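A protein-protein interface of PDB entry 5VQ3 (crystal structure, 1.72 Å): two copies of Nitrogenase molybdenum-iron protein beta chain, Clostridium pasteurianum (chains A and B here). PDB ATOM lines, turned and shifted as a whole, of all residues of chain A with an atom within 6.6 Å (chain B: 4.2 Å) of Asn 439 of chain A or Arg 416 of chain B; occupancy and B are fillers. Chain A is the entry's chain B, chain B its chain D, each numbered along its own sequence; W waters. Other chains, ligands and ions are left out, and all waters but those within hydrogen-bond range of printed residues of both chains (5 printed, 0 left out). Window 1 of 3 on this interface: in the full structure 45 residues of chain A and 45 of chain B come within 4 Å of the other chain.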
ATOM      1  N   VAL A 434     -12.417  -3.215 -17.323  1.00  0.00           N
ATOM      2  CA  VAL A 434     -11.096  -3.179 -16.732  1.00  0.00           C
ATOM      3  C   VAL A 434     -10.831  -4.485 -15.995  1.00  0.00           C
ATOM      4  O   VAL A 434      -9.724  -4.988 -16.025  1.00  0.00           O
ATOM      5  CB  VAL A 434     -10.923  -1.976 -15.821  1.00  0.00           C
ATOM      6  CG1 VAL A 434      -9.576  -2.040 -15.075  1.00  0.00           C
ATOM      7  CG2 VAL A 434     -11.029  -0.676 -16.628  1.00  0.00           C
ATOM      8  N   GLU A 435     -11.869  -5.052 -15.378  1.00  0.00           N
ATOM      9  CA  GLU A 435     -11.749  -6.350 -14.739  1.00  0.00           C
ATOM     10  C   GLU A 435     -11.405  -7.435 -15.769  1.00  0.00           C
ATOM     11  O   GLU A 435     -10.514  -8.230 -15.533  1.00  0.00           O
ATOM     12  CB  GLU A 435     -13.077  -6.761 -14.071  1.00  0.00           C
ATOM     13  CG  GLU A 435     -13.413  -5.958 -12.845  1.00  0.00           C
ATOM     14  CD  GLU A 435     -14.803  -6.287 -12.285  1.00  0.00           C
ATOM     15  OE1 GLU A 435     -15.631  -6.919 -12.985  1.00  0.00           O
ATOM     16  OE2 GLU A 435     -15.069  -5.863 -11.151  1.00  0.00           O
ATOM     17  N   GLU A 436     -12.096  -7.429 -16.907  1.00  0.00           N
ATOM     18  CA  GLU A 436     -11.865  -8.442 -17.951  1.00  0.00           C
ATOM     19  C   GLU A 436     -10.459  -8.325 -18.485  1.00  0.00           C
ATOM     20  O   GLU A 436      -9.786  -9.314 -18.638  1.00  0.00           O
ATOM     21  CB  GLU A 436     -12.856  -8.290 -19.104  1.00  0.00           C
ATOM     22  CG  GLU A 436     -14.236  -8.847 -18.838  1.00  0.00           C
ATOM     23  CD  GLU A 436     -15.135  -8.691 -20.071  1.00  0.00           C
ATOM     24  OE1 GLU A 436     -15.285  -7.542 -20.602  1.00  0.00           O
ATOM     25  OE2 GLU A 436     -15.674  -9.725 -20.521  1.00  0.00           O
ATOM     26  N   ILE A 437     -10.032  -7.085 -18.762  1.00  0.00           N
ATOM     27  CA  ILE A 437      -8.723  -6.832 -19.362  1.00  0.00           C
ATOM     28  C   ILE A 437      -7.634  -7.281 -18.414  1.00  0.00           C
ATOM     29  O   ILE A 437      -6.734  -8.050 -18.789  1.00  0.00           O
ATOM     30  CB  ILE A 437      -8.552  -5.364 -19.766  1.00  0.00           C
ATOM     31  CG1 ILE A 437      -9.412  -5.057 -20.991  1.00  0.00           C
ATOM     32  CG2 ILE A 437      -7.081  -5.051 -20.018  1.00  0.00           C
ATOM     33  CD1 ILE A 437      -9.626  -3.570 -21.219  1.00  0.00           C
ATOM     34  N   THR A 438      -7.727  -6.861 -17.156  1.00  0.00           N
ATOM     35  CA  THR A 438      -6.691  -7.206 -16.229  1.00  0.00           C
ATOM     36  C   THR A 438      -6.706  -8.699 -15.918  1.00  0.00           C
ATOM     37  O   THR A 438      -5.649  -9.326 -15.770  1.00  0.00           O
ATOM     38  CB  THR A 438      -6.714  -6.342 -14.961  1.00  0.00           C
ATOM     39  OG1 THR A 438      -7.961  -6.463 -14.294  1.00  0.00           O
ATOM     40  CG2 THR A 438      -6.514  -4.913 -15.322  1.00  0.00           C
ATOM     41  N   ASN A 439      -7.882  -9.296 -15.841  1.00  0.00           N
ATOM     42  CA  ASN A 439      -8.003 -10.731 -15.620  1.00  0.00           C
ATOM     43  C   ASN A 439      -7.275 -11.547 -16.713  1.00  0.00           C
ATOM     44  O   ASN A 439      -6.540 -12.468 -16.377  1.00  0.00           O
ATOM     45  CB  ASN A 439      -9.476 -11.188 -15.580  1.00  0.00           C
ATOM     46  CG  ASN A 439     -10.174 -10.898 -14.231  1.00  0.00           C
ATOM     47  OD1 ASN A 439      -9.564 -10.461 -13.263  1.00  0.00           O
ATOM     48  ND2 ASN A 439     -11.447 -11.172 -14.184  1.00  0.00           N
ATOM     49  N   VAL A 440      -7.463 -11.211 -17.992  1.00  0.00           N
ATOM     50  CA  VAL A 440      -6.838 -12.018 -19.070  1.00  0.00           C
ATOM     51  C   VAL A 440      -5.324 -11.767 -19.133  1.00  0.00           C
ATOM     52  O   VAL A 440      -4.553 -12.700 -19.381  1.00  0.00           O
ATOM     53  CB  VAL A 440      -7.514 -11.857 -20.473  1.00  0.00           C
ATOM     54  CG1 VAL A 440      -8.986 -12.231 -20.447  1.00  0.00           C
ATOM     55  CG2 VAL A 440      -7.431 -10.449 -20.975  1.00  0.00           C
ATOM     56  N   ILE A 441      -4.898 -10.541 -18.834  1.00  0.00           N
ATOM     57  CA  ILE A 441      -3.461 -10.193 -18.722  1.00  0.00           C
ATOM     58  C   ILE A 441      -2.779 -10.980 -17.593  1.00  0.00           C
ATOM     59  O   ILE A 441      -1.781 -11.649 -17.808  1.00  0.00           O
ATOM     60  CB  ILE A 441      -3.258  -8.686 -18.597  1.00  0.00           C
ATOM     61  CG1 ILE A 441      -3.513  -8.044 -19.971  1.00  0.00           C
ATOM     62  CG2 ILE A 441      -1.853  -8.327 -18.138  1.00  0.00           C
ATOM     63  CD1 ILE A 441      -3.616  -6.546 -19.948  1.00  0.00           C
ATOM     64  N   LEU A 442      -3.381 -10.946 -16.419  1.00  0.00           N
ATOM     65  CA  LEU A 442      -2.827 -11.669 -15.248  1.00  0.00           C
ATOM     66  C   LEU A 442      -2.913 -13.187 -15.412  1.00  0.00           C
ATOM     67  O   LEU A 442      -2.006 -13.886 -15.013  1.00  0.00           O
ATOM     68  CB  LEU A 442      -3.516 -11.232 -13.957  1.00  0.00           C
ATOM     69  CG  LEU A 442      -3.056  -9.841 -13.505  1.00  0.00           C
ATOM     70  CD1 LEU A 442      -4.042  -9.226 -12.540  1.00  0.00           C
ATOM     71  CD2 LEU A 442      -1.676  -9.920 -12.860  1.00  0.00           C
ATOM     72  N   ASP A 443      -3.991 -13.707 -16.006  1.00  0.00           N
ATOM     73  CA  ASP A 443      -4.094 -15.164 -16.260  1.00  0.00           C
ATOM     74  C   ASP A 443      -2.925 -15.681 -17.102  1.00  0.00           C
ATOM     75  O   ASP A 443      -2.358 -16.738 -16.826  1.00  0.00           O
ATOM     76  CB  ASP A 443      -5.384 -15.503 -17.018  1.00  0.00           C
ATOM     77  CG  ASP A 443      -6.622 -15.568 -16.122  1.00  0.00           C
ATOM     78  OD1 ASP A 443      -6.515 -15.625 -14.861  1.00  0.00           O
ATOM     79  OD2 ASP A 443      -7.726 -15.614 -16.707  1.00  0.00           O
ATOM     80  N   LYS A 444      -2.571 -14.939 -18.138  1.00  0.00           N
ATOM     81  CA  LYS A 444      -1.431 -15.308 -18.972  1.00  0.00           C
ATOM     82  C   LYS A 444      -0.100 -15.227 -18.236  1.00  0.00           C
ATOM     83  O   LYS A 444       0.669 -16.162 -18.296  1.00  0.00           O
ATOM     84  CB  LYS A 444      -1.370 -14.497 -20.251  1.00  0.00           C
ATOM     85  CG  LYS A 444      -0.110 -14.835 -21.046  1.00  0.00           C
ATOM     86  CD  LYS A 444       0.006 -14.071 -22.332  1.00  0.00           C
ATOM     87  CE  LYS A 444       1.168 -14.655 -23.159  1.00  0.00           C
ATOM     88  NZ  LYS A 444       1.349 -13.850 -24.378  1.00  0.00           N
ATOM     89  N   GLU A 446       0.393 -15.581 -15.075  1.00  0.00           N
ATOM     90  CA  GLU A 446       0.472 -16.644 -14.071  1.00  0.00           C
ATOM     91  C   GLU A 446       0.544 -18.044 -14.654  1.00  0.00           C
ATOM     92  O   GLU A 446       1.029 -18.943 -13.984  1.00  0.00           O
ATOM     93  CB  GLU A 446      -0.651 -16.500 -13.041  1.00  0.00           C
ATOM     94  CG  GLU A 446      -0.579 -15.094 -12.399  1.00  0.00           C
ATOM     95  CD  GLU A 446      -1.248 -14.969 -11.045  1.00  0.00           C
ATOM     96  OE1 GLU A 446      -0.584 -14.553 -10.056  1.00  0.00           O
ATOM     97  OE2 GLU A 446      -2.415 -15.287 -10.989  1.00  0.00           O
ATOM     98  N   ARG A 458      -0.907  -9.964  -6.436  1.00  0.00           N
ATOM     99  CA  ARG A 458      -0.682  -9.230  -7.691  1.00  0.00           C
ATOM    100  C   ARG A 458      -1.326  -7.887  -7.583  1.00  0.00           C
ATOM    101  O   ARG A 458      -0.992  -6.966  -8.367  1.00  0.00           O
ATOM    102  CB  ARG A 458      -1.238  -9.956  -8.882  1.00  0.00           C
ATOM    103  CG  ARG A 458      -0.520 -11.268  -9.183  1.00  0.00           C
ATOM    104  CD  ARG A 458       0.727 -11.106  -9.993  1.00  0.00           C
ATOM    105  NE  ARG A 458       1.217 -12.428 -10.416  1.00  0.00           N
ATOM    106  CZ  ARG A 458       2.382 -12.612 -11.035  1.00  0.00           C
ATOM    107  NH1 ARG A 458       3.171 -11.560 -11.336  1.00  0.00           N
ATOM    108  NH2 ARG A 458       2.772 -13.848 -11.350  1.00  0.00           N
ATOM    109  OXT ARG A 458      -2.182  -7.724  -6.702  1.00  0.00           O
ATOM    110  N   ARG B 408     -11.862 -17.778  -8.223  1.00  0.00           N
ATOM    111  CA  ARG B 408     -11.560 -17.137  -6.956  1.00  0.00           C
ATOM    112  C   ARG B 408     -12.854 -16.755  -6.276  1.00  0.00           C
ATOM    113  O   ARG B 408     -13.755 -16.158  -6.879  1.00  0.00           O
ATOM    114  CB  ARG B 408     -10.677 -15.909  -7.193  1.00  0.00           C
ATOM    115  CG  ARG B 408      -9.302 -16.273  -7.696  1.00  0.00           C
ATOM    116  CD  ARG B 408      -8.619 -15.065  -8.321  1.00  0.00           C
ATOM    117  NE  ARG B 408      -7.209 -15.365  -8.535  1.00  0.00           N
ATOM    118  CZ  ARG B 408      -6.767 -16.066  -9.562  1.00  0.00           C
ATOM    119  NH1 ARG B 408      -7.631 -16.529 -10.464  1.00  0.00           N
ATOM    120  NH2 ARG B 408      -5.485 -16.359  -9.655  1.00  0.00           N
ATOM    121  N   MET B 414      -6.343 -11.816  -3.405  1.00  0.00           N
ATOM    122  CA  MET B 414      -5.304 -10.811  -3.338  1.00  0.00           C
ATOM    123  C   MET B 414      -4.604 -10.608  -4.668  1.00  0.00           C
ATOM    124  O   MET B 414      -3.628  -9.871  -4.736  1.00  0.00           O
ATOM    125  CB  MET B 414      -4.284 -11.190  -2.280  1.00  0.00           C
ATOM    126  CG  MET B 414      -4.894 -11.295  -0.892  1.00  0.00           C
ATOM    127  SD  MET B 414      -3.744 -11.725   0.409  1.00  0.00           S
ATOM    128  CE  MET B 414      -3.450 -13.419   0.017  1.00  0.00           C
ATOM    129  N   ASP B 415      -5.083 -11.279  -5.711  1.00  0.00           N
ATOM    130  CA  ASP B 415      -4.343 -11.303  -6.970  1.00  0.00           C
ATOM    131  C   ASP B 415      -5.128 -10.884  -8.201  1.00  0.00           C
ATOM    132  O   ASP B 415      -4.681 -11.083  -9.315  1.00  0.00           O
ATOM    133  CB  ASP B 415      -3.667 -12.653  -7.176  1.00  0.00           C
ATOM    134  CG  ASP B 415      -4.630 -13.800  -7.160  1.00  0.00           C
ATOM    135  OD1 ASP B 415      -5.781 -13.622  -6.696  1.00  0.00           O
ATOM    136  OD2 ASP B 415      -4.215 -14.918  -7.560  1.00  0.00           O
ATOM    137  N   ARG B 416      -6.275 -10.257  -7.998  1.00  0.00           N
ATOM    138  CA  ARG B 416      -7.087  -9.733  -9.109  1.00  0.00           C
ATOM    139  C   ARG B 416      -7.692  -8.402  -8.683  1.00  0.00           C
ATOM    140  O   ARG B 416      -7.736  -8.061  -7.477  1.00  0.00           O
ATOM    141  CB  ARG B 416      -8.190 -10.724  -9.535  1.00  0.00           C
ATOM    142  CG  ARG B 416      -7.717 -12.028 -10.255  1.00  0.00           C
ATOM    143  CD  ARG B 416      -6.890 -11.771 -11.518  1.00  0.00           C
ATOM    144  NE  ARG B 416      -6.427 -13.000 -12.200  1.00  0.00           N
ATOM    145  CZ  ARG B 416      -5.298 -13.645 -11.955  1.00  0.00           C
ATOM    146  NH1 ARG B 416      -4.429 -13.257 -10.999  1.00  0.00           N
ATOM    147  NH2 ARG B 416      -4.999 -14.730 -12.687  1.00  0.00           N
ATOM    148  N   TYR B 417      -8.137  -7.634  -9.665  1.00  0.00           N
ATOM    149  CA  TYR B 417      -8.580  -6.266  -9.401  1.00  0.00           C
ATOM    150  C   TYR B 417     -10.041  -6.116  -9.684  1.00  0.00           C
ATOM    151  O   TYR B 417     -10.505  -6.544 -10.732  1.00  0.00           O
ATOM    152  CB  TYR B 417      -7.775  -5.293 -10.253  1.00  0.00           C
ATOM    153  CG  TYR B 417      -6.368  -5.181  -9.761  1.00  0.00           C
ATOM    154  CD1 TYR B 417      -5.413  -6.089 -10.128  1.00  0.00           C
ATOM    155  CD2 TYR B 417      -6.024  -4.198  -8.840  1.00  0.00           C
ATOM    156  CE1 TYR B 417      -4.118  -6.035  -9.607  1.00  0.00           C
ATOM    157  CE2 TYR B 417      -4.767  -4.130  -8.323  1.00  0.00           C
ATOM    158  CZ  TYR B 417      -3.796  -5.040  -8.707  1.00  0.00           C
ATOM    159  OH  TYR B 417      -2.515  -4.923  -8.164  1.00  0.00           O
ATOM    160  N   GLY B 418     -10.769  -5.541  -8.733  1.00  0.00           N
ATOM    161  CA  GLY B 418     -12.184  -5.200  -8.945  1.00  0.00           C
ATOM    162  C   GLY B 418     -13.194  -6.243  -8.518  1.00  0.00           C
ATOM    163  O   GLY B 418     -14.415  -6.001  -8.613  1.00  0.00           O
ATOM    164  N   HIS B 419     -12.732  -7.408  -8.029  1.00  0.00           N
ATOM    165  CA  HIS B 419     -13.647  -8.472  -7.520  1.00  0.00           C
ATOM    166  C   HIS B 419     -14.551  -8.000  -6.400  1.00  0.00           C
ATOM    167  O   HIS B 419     -15.677  -8.462  -6.290  1.00  0.00           O
ATOM    168  CB  HIS B 419     -12.867  -9.733  -7.046  1.00  0.00           C
ATOM    169  CG  HIS B 419     -11.840  -9.448  -6.005  1.00  0.00           C
ATOM    170  ND1 HIS B 419     -12.111  -9.448  -4.655  1.00  0.00           N
ATOM    171  CD2 HIS B 419     -10.528  -9.127  -6.124  1.00  0.00           C
ATOM    172  CE1 HIS B 419     -11.004  -9.144  -3.988  1.00  0.00           C
ATOM    173  NE2 HIS B 419     -10.042  -8.928  -4.864  1.00  0.00           N
HETATM  174  O   HOH W   1      -3.698 -17.778 -11.485  1.00  0.00           O
HETATM  175  O   HOH W   2      -8.527 -14.015 -13.762  1.00  0.00           O
HETATM  176  O   HOH W   3     -11.175  -9.127 -11.468  1.00  0.00           O
HETATM  177  O   HOH W   4      -7.874  -8.479 -12.376  1.00  0.00           O
HETATM  178  O   HOH W   5      -6.726 -17.804 -12.994  1.00  0.00           O
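No position is printed for both chains. Of the 12 pairs that touch across the chains among the printed residues, none has its exchanged pair printed and touching as well.
OD1 of Asp 443 of chain A is in salt-bridge range of NH2 of Arg 416 of chain B (2.8 Å). The side-chain carboxylate of Glu 435 of chain A lies close to the backbone carbonyl oxygen of Gly 418 of chain B. The chain-end carboxylate of Arg 458 of chain A lies within hydrogen-bond range of the side-chain hydroxyl of Tyr 417 of chain B, at 2.6 Å. The side-chain carboxylate (OE2) of Glu 446 of chain A lies within salt-bridge range of the guanidinium group (NH1) of Arg 416 of chain B. The side-chain carboxylate (OE2) of Glu 446 of chain A lies within salt-bridge range of the guanidinium group (NH2) of Arg 408 of chain B, 3.5 Å away. O of Met 414 of chain B sits at hydrogen-bond distance from N of Arg 458 of chain A, 3.2 Å away.
Among the printed residues, merely in contact across the chains: Asn 439 of chain A with Arg 416 of chain B (3.5 Å), Leu 442 of chain A with Arg 416 of chain B (3.6 Å), Glu 435 of chain A with Tyr 417 of chain B (3.6 Å), Arg 458 of chain A with Asp 415 of chain B (3.6 Å), Leu 442 of chain A with Asp 415 of chain B (3.8 Å) and Glu 446 of chain A with Asp 415 of chain B (3.9 Å).
Water W4 lies within hydrogen-bond range of OD1 of Asn 439 of chain A, OG1 of Thr 438 of chain A and N of Tyr 417 of chain B. Water W3 lies within hydrogen-bond range of the side-chain amide oxygen of Asn 439 of chain A and the backbone carbonyl oxygen of Tyr 417 of chain B. Water W2 bridges the side-chain carboxylate (OD1) of Asp 443 of chain A (2.8 Å) and the guanidinium group (NE) of Arg 416 of chain B (2.8 Å). Water W1 bridges OE2 of Glu 446 of chain A (2.8 Å) and NH2 of Arg 408 of chain B (2.9 Å). Water W5 bridges the side-chain carboxylate of Asp 443 of chain A and the guanidinium group of Arg 408 of chain B.
Asn 439 of chain A touches just one residue of chain B: Arg 416. Of the printed residues of chain B, Asp 443 of chain A touches Arg 416 (2.8 Å). Of the printed residues of chain B, Arg 458 of chain A touches Met 414 (3.2 Å), Asp 415 (3.6 Å) and Tyr 417 (2.6 Å). Of the printed residues of chain A, Met 414 of chain B touches Arg 458 (3.2 Å). Arg 416 of chain B touches just these residues of chain A: Asn 439, Leu 442, Asp 443 and Glu 446. Of the printed residues of chain A, Gly 418 of chain B touches Glu 435 (2.6 Å). The nearest printed residue of chain B that does not touch Arg 458 of chain A is Arg 416 of chain B (4.7 Å).
OE1 of Glu 446 of chain A lies within salt-bridge range of NE of Arg 458 of chain A (2.8 Å). The guanidinium group (NH2) of Arg 408 of chain B lies within salt-bridge range of the side-chain carboxylate (OD2) of Asp 415 of chain B (2.8 Å). OG1 of Thr 438 of chain A sits at hydrogen-bond distance from O of Glu 435 of chain A (3.3 Å). OD2 of Asp 415 of chain B lies within salt-bridge range of NH1 of Arg 416 of chain B, 3.8 Å away. The side-chain amide oxygen of Asn 439 of chain A sits close to the backbone carbonyl oxygen of Glu 435 of chain A (3.3 Å).
Of the 13 printed residues of chain A, 6 touch a printed residue of chain B. Printed residues of chain A that touch a printed residue of chain B: Glu 435, Asn 439, Leu 442, Asp 443, Glu 446 and Arg 458. Along chain A the printed residues that touch a printed residue of chain B span positions 435 to 458.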
